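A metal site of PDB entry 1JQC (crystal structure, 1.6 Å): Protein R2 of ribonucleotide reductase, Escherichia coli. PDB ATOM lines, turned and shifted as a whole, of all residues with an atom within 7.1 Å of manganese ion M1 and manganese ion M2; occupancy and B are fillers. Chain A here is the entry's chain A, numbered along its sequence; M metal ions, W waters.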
ATOM      1  N   GLN A  80      23.072   8.814  13.671  1.00  0.00           N
ATOM      2  CA  GLN A  80      24.356   8.109  13.761  1.00  0.00           C
ATOM      3  C   GLN A  80      25.146   8.637  14.956  1.00  0.00           C
ATOM      4  O   GLN A  80      25.742   7.853  15.734  1.00  0.00           O
ATOM      5  CB  GLN A  80      25.166   8.315  12.456  1.00  0.00           C
ATOM      6  CG  GLN A  80      24.421   7.636  11.264  1.00  0.00           C
ATOM      7  CD  GLN A  80      25.030   7.922   9.897  1.00  0.00           C
ATOM      8  OE1 GLN A  80      25.560   9.007   9.643  1.00  0.00           O
ATOM      9  NE2 GLN A  80      24.936   6.930   9.006  1.00  0.00           N
ATOM     10  N   LEU A  83      23.649   7.266  18.244  1.00  0.00           N
ATOM     11  CA  LEU A  83      23.995   5.864  18.472  1.00  0.00           C
ATOM     12  C   LEU A  83      25.459   5.654  18.881  1.00  0.00           C
ATOM     13  O   LEU A  83      25.746   4.883  19.837  1.00  0.00           O
ATOM     14  CB  LEU A  83      23.670   5.038  17.216  1.00  0.00           C
ATOM     15  CG  LEU A  83      22.156   4.857  16.976  1.00  0.00           C
ATOM     16  CD1 LEU A  83      22.023   3.889  15.827  1.00  0.00           C
ATOM     17  CD2 LEU A  83      21.422   4.283  18.162  1.00  0.00           C
ATOM     18  N   ASP A  84      26.393   6.362  18.237  1.00  0.00           N
ATOM     19  CA  ASP A  84      27.806   6.175  18.551  1.00  0.00           C
ATOM     20  C   ASP A  84      28.165   6.856  19.869  1.00  0.00           C
ATOM     21  O   ASP A  84      29.123   6.439  20.518  1.00  0.00           O
ATOM     22  CB  ASP A  84      28.748   6.647  17.424  1.00  0.00           C
ATOM     23  CG  ASP A  84      28.946   5.577  16.331  1.00  0.00           C
ATOM     24  OD1 ASP A  84      29.422   4.486  16.646  1.00  0.00           O
ATOM     25  OD2 ASP A  84      28.631   5.812  15.132  1.00  0.00           O
ATOM     26  N   GLN A  87      27.216   4.144  22.115  1.00  0.00           N
ATOM     27  CA  GLN A  87      28.093   2.985  21.970  1.00  0.00           C
ATOM     28  C   GLN A  87      29.539   3.231  22.378  1.00  0.00           C
ATOM     29  O   GLN A  87      30.251   2.253  22.641  1.00  0.00           O
ATOM     30  CB  GLN A  87      28.050   2.458  20.524  1.00  0.00           C
ATOM     31  CG  GLN A  87      26.687   1.822  20.218  1.00  0.00           C
ATOM     32  CD  GLN A  87      26.478   0.575  21.086  1.00  0.00           C
ATOM     33  OE1 GLN A  87      26.951  -0.514  20.740  1.00  0.00           O
ATOM     34  NE2 GLN A  87      25.817   0.750  22.167  1.00  0.00           N
ATOM     35  N   GLY A  88      29.970   4.483  22.452  1.00  0.00           N
ATOM     36  CA  GLY A  88      31.348   4.713  22.913  1.00  0.00           C
ATOM     37  C   GLY A  88      31.493   4.416  24.402  1.00  0.00           C
ATOM     38  O   GLY A  88      32.459   3.780  24.842  1.00  0.00           O
ATOM     39  N   TRP A 111      36.375  -2.360  20.971  1.00  0.00           N
ATOM     40  CA  TRP A 111      35.143  -2.058  20.291  1.00  0.00           C
ATOM     41  C   TRP A 111      34.636  -0.668  20.757  1.00  0.00           C
ATOM     42  O   TRP A 111      34.354   0.199  19.923  1.00  0.00           O
ATOM     43  CB  TRP A 111      34.152  -3.170  20.690  1.00  0.00           C
ATOM     44  CG  TRP A 111      32.677  -2.961  20.411  1.00  0.00           C
ATOM     45  CD1 TRP A 111      32.076  -2.091  19.541  1.00  0.00           C
ATOM     46  CD2 TRP A 111      31.632  -3.726  21.011  1.00  0.00           C
ATOM     47  NE1 TRP A 111      30.695  -2.295  19.575  1.00  0.00           N
ATOM     48  CE2 TRP A 111      30.418  -3.294  20.484  1.00  0.00           C
ATOM     49  CE3 TRP A 111      31.627  -4.749  21.985  1.00  0.00           C
ATOM     50  CZ2 TRP A 111      29.184  -3.862  20.885  1.00  0.00           C
ATOM     51  CZ3 TRP A 111      30.427  -5.296  22.397  1.00  0.00           C
ATOM     52  CH2 TRP A 111      29.217  -4.851  21.845  1.00  0.00           C
ATOM     53  N   SER A 114      36.692   2.107  19.357  1.00  0.00           N
ATOM     54  CA  SER A 114      36.454   2.311  17.930  1.00  0.00           C
ATOM     55  C   SER A 114      35.189   3.162  17.721  1.00  0.00           C
ATOM     56  O   SER A 114      35.124   3.947  16.777  1.00  0.00           O
ATOM     57  CB  SER A 114      36.412   0.957  17.176  1.00  0.00           C
ATOM     58  OG  SER A 114      35.167   0.331  17.343  1.00  0.00           O
ATOM     59  N   GLU A 115      34.209   3.084  18.641  1.00  0.00           N
ATOM     60  CA  GLU A 115      33.007   3.888  18.515  1.00  0.00           C
ATOM     61  C   GLU A 115      33.323   5.383  18.802  1.00  0.00           C
ATOM     62  O   GLU A 115      32.680   6.278  18.221  1.00  0.00           O
ATOM     63  CB  GLU A 115      31.941   3.400  19.504  1.00  0.00           C
ATOM     64  CG  GLU A 115      31.554   1.907  19.421  1.00  0.00           C
ATOM     65  CD  GLU A 115      30.830   1.504  18.178  1.00  0.00           C
ATOM     66  OE1 GLU A 115      31.056   2.163  17.144  1.00  0.00           O
ATOM     67  OE2 GLU A 115      30.099   0.534  18.216  1.00  0.00           O
ATOM     68  N   THR A 116      34.280   5.669  19.694  1.00  0.00           N
ATOM     69  CA  THR A 116      34.657   7.070  19.953  1.00  0.00           C
ATOM     70  C   THR A 116      35.292   7.646  18.702  1.00  0.00           C
ATOM     71  O   THR A 116      35.173   8.835  18.480  1.00  0.00           O
ATOM     72  CB  THR A 116      35.627   7.265  21.176  1.00  0.00           C
ATOM     73  OG1 THR A 116      36.920   6.729  20.870  1.00  0.00           O
ATOM     74  CG2 THR A 116      35.023   6.546  22.432  1.00  0.00           C
ATOM     75  N   HIS A 118      34.320   6.810  15.734  1.00  0.00           N
ATOM     76  CA  HIS A 118      33.142   7.129  14.883  1.00  0.00           C
ATOM     77  C   HIS A 118      32.562   8.480  15.339  1.00  0.00           C
ATOM     78  O   HIS A 118      32.244   9.370  14.495  1.00  0.00           O
ATOM     79  CB  HIS A 118      32.080   6.011  14.985  1.00  0.00           C
ATOM     80  CG  HIS A 118      32.577   4.693  14.518  1.00  0.00           C
ATOM     81  ND1 HIS A 118      31.836   3.546  14.609  1.00  0.00           N
ATOM     82  CD2 HIS A 118      33.741   4.352  13.940  1.00  0.00           C
ATOM     83  CE1 HIS A 118      32.526   2.550  14.098  1.00  0.00           C
ATOM     84  NE2 HIS A 118      33.684   3.015  13.689  1.00  0.00           N
ATOM     85  N   SER A 119      32.405   8.697  16.645  1.00  0.00           N
ATOM     86  CA  SER A 119      31.882   9.990  17.085  1.00  0.00           C
ATOM     87  C   SER A 119      32.755  11.148  16.635  1.00  0.00           C
ATOM     88  O   SER A 119      32.246  12.202  16.259  1.00  0.00           O
ATOM     89  CB  SER A 119      31.776  10.018  18.630  1.00  0.00           C
ATOM     90  OG  SER A 119      30.859   9.044  19.047  1.00  0.00           O
ATOM     91  N   TYR A 122      32.016  12.140  13.140  1.00  0.00           N
ATOM     92  CA  TYR A 122      30.813  12.969  12.929  1.00  0.00           C
ATOM     93  C   TYR A 122      31.103  14.430  13.259  1.00  0.00           C
ATOM     94  O   TYR A 122      30.553  15.319  12.607  1.00  0.00           O
ATOM     95  CB  TYR A 122      29.634  12.484  13.769  1.00  0.00           C
ATOM     96  CG  TYR A 122      29.329  11.023  13.545  1.00  0.00           C
ATOM     97  CD1 TYR A 122      29.282  10.491  12.243  1.00  0.00           C
ATOM     98  CD2 TYR A 122      29.079  10.173  14.628  1.00  0.00           C
ATOM     99  CE1 TYR A 122      28.985   9.125  12.043  1.00  0.00           C
ATOM    100  CE2 TYR A 122      28.776   8.851  14.436  1.00  0.00           C
ATOM    101  CZ  TYR A 122      28.730   8.310  13.171  1.00  0.00           C
ATOM    102  OH  TYR A 122      28.393   6.969  12.969  1.00  0.00           O
ATOM    103  N   VAL A 200      21.897  -4.934  21.588  1.00  0.00           N
ATOM    104  CA  VAL A 200      23.090  -4.350  20.941  1.00  0.00           C
ATOM    105  C   VAL A 200      23.284  -4.953  19.548  1.00  0.00           C
ATOM    106  O   VAL A 200      23.627  -4.242  18.573  1.00  0.00           O
ATOM    107  CB  VAL A 200      24.335  -4.602  21.792  1.00  0.00           C
ATOM    108  CG1 VAL A 200      25.589  -4.030  21.107  1.00  0.00           C
ATOM    109  CG2 VAL A 200      24.157  -3.926  23.140  1.00  0.00           C
ATOM    110  N   LEU A 203      21.012  -3.183  17.345  1.00  0.00           N
ATOM    111  CA  LEU A 203      21.475  -1.859  17.136  1.00  0.00           C
ATOM    112  C   LEU A 203      22.580  -1.849  16.073  1.00  0.00           C
ATOM    113  O   LEU A 203      22.510  -1.086  15.133  1.00  0.00           O
ATOM    114  CB  LEU A 203      22.033  -1.307  18.471  1.00  0.00           C
ATOM    115  CG  LEU A 203      22.472   0.172  18.513  1.00  0.00           C
ATOM    116  CD1 LEU A 203      22.672   0.528  20.003  1.00  0.00           C
ATOM    117  CD2 LEU A 203      23.832   0.448  17.781  1.00  0.00           C
ATOM    118  N   GLU A 204      23.569  -2.714  16.202  1.00  0.00           N
ATOM    119  CA  GLU A 204      24.630  -2.537  15.213  1.00  0.00           C
ATOM    120  C   GLU A 204      24.322  -3.200  13.890  1.00  0.00           C
ATOM    121  O   GLU A 204      24.754  -2.724  12.834  1.00  0.00           O
ATOM    122  CB  GLU A 204      25.936  -3.016  15.802  1.00  0.00           C
ATOM    123  CG  GLU A 204      26.361  -2.110  16.957  1.00  0.00           C
ATOM    124  CD  GLU A 204      27.649  -2.528  17.545  1.00  0.00           C
ATOM    125  OE1 GLU A 204      27.791  -3.723  17.801  1.00  0.00           O
ATOM    126  OE2 GLU A 204      28.487  -1.647  17.788  1.00  0.00           O
ATOM    127  N   PHE A 208      22.104   0.628  12.488  1.00  0.00           N
ATOM    128  CA  PHE A 208      23.189   1.328  11.799  1.00  0.00           C
ATOM    129  C   PHE A 208      23.170   1.085  10.290  1.00  0.00           C
ATOM    130  O   PHE A 208      23.479   2.007   9.515  1.00  0.00           O
ATOM    131  CB  PHE A 208      24.543   0.952  12.382  1.00  0.00           C
ATOM    132  CG  PHE A 208      25.152   2.054  13.185  1.00  0.00           C
ATOM    133  CD1 PHE A 208      25.358   3.294  12.586  1.00  0.00           C
ATOM    134  CD2 PHE A 208      25.408   1.913  14.536  1.00  0.00           C
ATOM    135  CE1 PHE A 208      25.812   4.398  13.323  1.00  0.00           C
ATOM    136  CE2 PHE A 208      25.858   3.003  15.297  1.00  0.00           C
ATOM    137  CZ  PHE A 208      26.057   4.248  14.683  1.00  0.00           C
ATOM    138  N   PHE A 212      23.209   3.590   7.073  1.00  0.00           N
ATOM    139  CA  PHE A 212      24.267   3.537   6.041  1.00  0.00           C
ATOM    140  C   PHE A 212      23.611   3.713   4.667  1.00  0.00           C
ATOM    141  O   PHE A 212      24.130   4.442   3.774  1.00  0.00           O
ATOM    142  CB  PHE A 212      25.029   2.198   6.095  1.00  0.00           C
ATOM    143  CG  PHE A 212      25.835   1.988   7.351  1.00  0.00           C
ATOM    144  CD1 PHE A 212      26.267   3.073   8.106  1.00  0.00           C
ATOM    145  CD2 PHE A 212      26.156   0.701   7.773  1.00  0.00           C
ATOM    146  CE1 PHE A 212      27.036   2.878   9.265  1.00  0.00           C
ATOM    147  CE2 PHE A 212      26.953   0.521   8.963  1.00  0.00           C
ATOM    148  CZ  PHE A 212      27.357   1.607   9.672  1.00  0.00           C
ATOM    149  N   ILE A 234      33.403   3.408   8.735  1.00  0.00           N
ATOM    150  CA  ILE A 234      32.541   3.052   9.910  1.00  0.00           C
ATOM    151  C   ILE A 234      31.831   1.721   9.693  1.00  0.00           C
ATOM    152  O   ILE A 234      31.763   0.844  10.626  1.00  0.00           O
ATOM    153  CB  ILE A 234      31.524   4.182  10.170  1.00  0.00           C
ATOM    154  CG1 ILE A 234      32.267   5.408  10.697  1.00  0.00           C
ATOM    155  CG2 ILE A 234      30.387   3.719  11.212  1.00  0.00           C
ATOM    156  CD1 ILE A 234      31.327   6.590  10.943  1.00  0.00           C
ATOM    157  N   ASP A 237      33.944  -1.215  10.363  1.00  0.00           N
ATOM    158  CA  ASP A 237      34.070  -1.476  11.812  1.00  0.00           C
ATOM    159  C   ASP A 237      32.804  -2.123  12.344  1.00  0.00           C
ATOM    160  O   ASP A 237      32.864  -3.071  13.126  1.00  0.00           O
ATOM    161  CB  ASP A 237      34.300  -0.178  12.615  1.00  0.00           C
ATOM    162  CG  ASP A 237      35.643   0.480  12.326  1.00  0.00           C
ATOM    163  OD1 ASP A 237      36.600  -0.224  11.931  1.00  0.00           O
ATOM    164  OD2 ASP A 237      35.726   1.687  12.588  1.00  0.00           O
ATOM    165  N   GLU A 238      31.641  -1.599  11.937  1.00  0.00           N
ATOM    166  CA  GLU A 238      30.397  -2.160  12.457  1.00  0.00           C
ATOM    167  C   GLU A 238      30.238  -3.626  12.106  1.00  0.00           C
ATOM    168  O   GLU A 238      29.652  -4.397  12.880  1.00  0.00           O
ATOM    169  CB  GLU A 238      29.172  -1.359  11.953  1.00  0.00           C
ATOM    170  CG  GLU A 238      29.078   0.062  12.631  1.00  0.00           C
ATOM    171  CD  GLU A 238      29.283  -0.015  14.168  1.00  0.00           C
ATOM    172  OE1 GLU A 238      28.731  -0.980  14.761  1.00  0.00           O
ATOM    173  OE2 GLU A 238      29.974   0.880  14.757  1.00  0.00           O
ATOM    174  N   ALA A 239      30.753  -4.044  10.925  1.00  0.00           N
ATOM    175  CA  ALA A 239      30.658  -5.458  10.533  1.00  0.00           C
ATOM    176  C   ALA A 239      31.408  -6.295  11.580  1.00  0.00           C
ATOM    177  O   ALA A 239      30.974  -7.389  11.944  1.00  0.00           O
ATOM    178  CB  ALA A 239      31.263  -5.649   9.119  1.00  0.00           C
ATOM    179  N   HIS A 241      31.852  -5.395  14.743  1.00  0.00           N
ATOM    180  CA  HIS A 241      31.096  -5.295  16.004  1.00  0.00           C
ATOM    181  C   HIS A 241      29.925  -6.271  16.012  1.00  0.00           C
ATOM    182  O   HIS A 241      29.684  -6.962  16.992  1.00  0.00           O
ATOM    183  CB  HIS A 241      30.594  -3.857  16.225  1.00  0.00           C
ATOM    184  CG  HIS A 241      31.690  -2.843  16.242  1.00  0.00           C
ATOM    185  ND1 HIS A 241      31.441  -1.468  16.230  1.00  0.00           N
ATOM    186  CD2 HIS A 241      33.022  -2.990  16.243  1.00  0.00           C
ATOM    187  CE1 HIS A 241      32.608  -0.836  16.251  1.00  0.00           C
ATOM    188  NE2 HIS A 241      33.571  -1.727  16.254  1.00  0.00           N
ATOM    189  N   LEU A 242      29.182  -6.315  14.926  1.00  0.00           N
ATOM    190  CA  LEU A 242      28.044  -7.246  14.925  1.00  0.00           C
ATOM    191  C   LEU A 242      28.545  -8.707  14.855  1.00  0.00           C
ATOM    192  O   LEU A 242      27.893  -9.644  15.365  1.00  0.00           O
ATOM    193  CB  LEU A 242      27.094  -6.866  13.776  1.00  0.00           C
ATOM    194  CG  LEU A 242      27.594  -7.134  12.383  1.00  0.00           C
ATOM    195  CD1 LEU A 242      27.167  -8.545  11.993  1.00  0.00           C
ATOM    196  CD2 LEU A 242      26.968  -6.124  11.400  1.00  0.00           C
HETATM  197 MN    MN M   1      29.960   2.938  15.564  1.00  0.00          MN
HETATM  198 MN    MN M   2      29.444  -0.381  16.463  1.00  0.00          MN
HETATM  199  O   HOH W   1      28.669   3.252  13.806  1.00  0.00           O
HETATM  200  O   HOH W   2      27.761   1.185  16.640  1.00  0.00           O
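OH of Tyr 122 lies within hydrogen-bond range of OD2 of Asp 84, 2.5 Å away.
O of Asp 84 is in hydrogen-bond range of OG of Ser 119.
OE2 of Glu 204 sits close to NE1 of Trp 111, at 2.9 Å.
The backbone carbonyl oxygen (O) of Glu 115 is in hydrogen-bond range of the side-chain hydroxyl (OG) of Ser 119, 3.4 Å away.
A ring nitrogen (NE2) of His 118 is in hydrogen-bond range of the side-chain carboxylate (OD2) of Asp 237, 2.7 Å away.
OG of Ser 114 lies within hydrogen-bond range of NE2 of His 241, 2.8 Å away.
O of Asp 237 sits close to NE2 of His 241 (3.5 Å).
The backbone carbonyl oxygen (O) of Trp 111 sits at hydrogen-bond distance from the side-chain hydroxyl (OG) of Ser 114 (2.7 Å).
Four residues have an atom within 4 Å of manganese ion M1: Asp 84, Glu 115, His 118 and Glu 238.
The nearest printed residue that does not touch manganese ion M1 is Phe 208 (4.1 Å).
Residues that only touch manganese ion M2: Trp 111 (3.9 Å).
Within 4 Å of manganese ion M2: Trp 111, Glu 115, Glu 204, Glu 238 and His 241.
OD1 of Asp 84 is bound to manganese ion M1, 2.0 Å away.
Manganese ion M1 is bound by OE1 of Glu 115 (2.1 Å).
ND1 of His 118 binds manganese ion M1, at 2.2 Å.
Water W1 is bound to manganese ion M1 (2.2 Å).
Manganese ion M1 is bound by the side-chain carboxylate (OE2) of Glu 238, at 2.2 Å.
Manganese ion M1 has five donor atoms within binding distance.
Manganese ion M2 is bound by OE1 of Glu 238 (1.9 Å), OE2 of Glu 204 (2.1 Å), OE2 of Glu 115 (2.1 Å), OE2 of Glu 238 (2.2 Å), ND1 of His 241 (2.3 Å) and water W2 (2.3 Å).
Manganese ion M2 has six donor atoms within binding distance.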
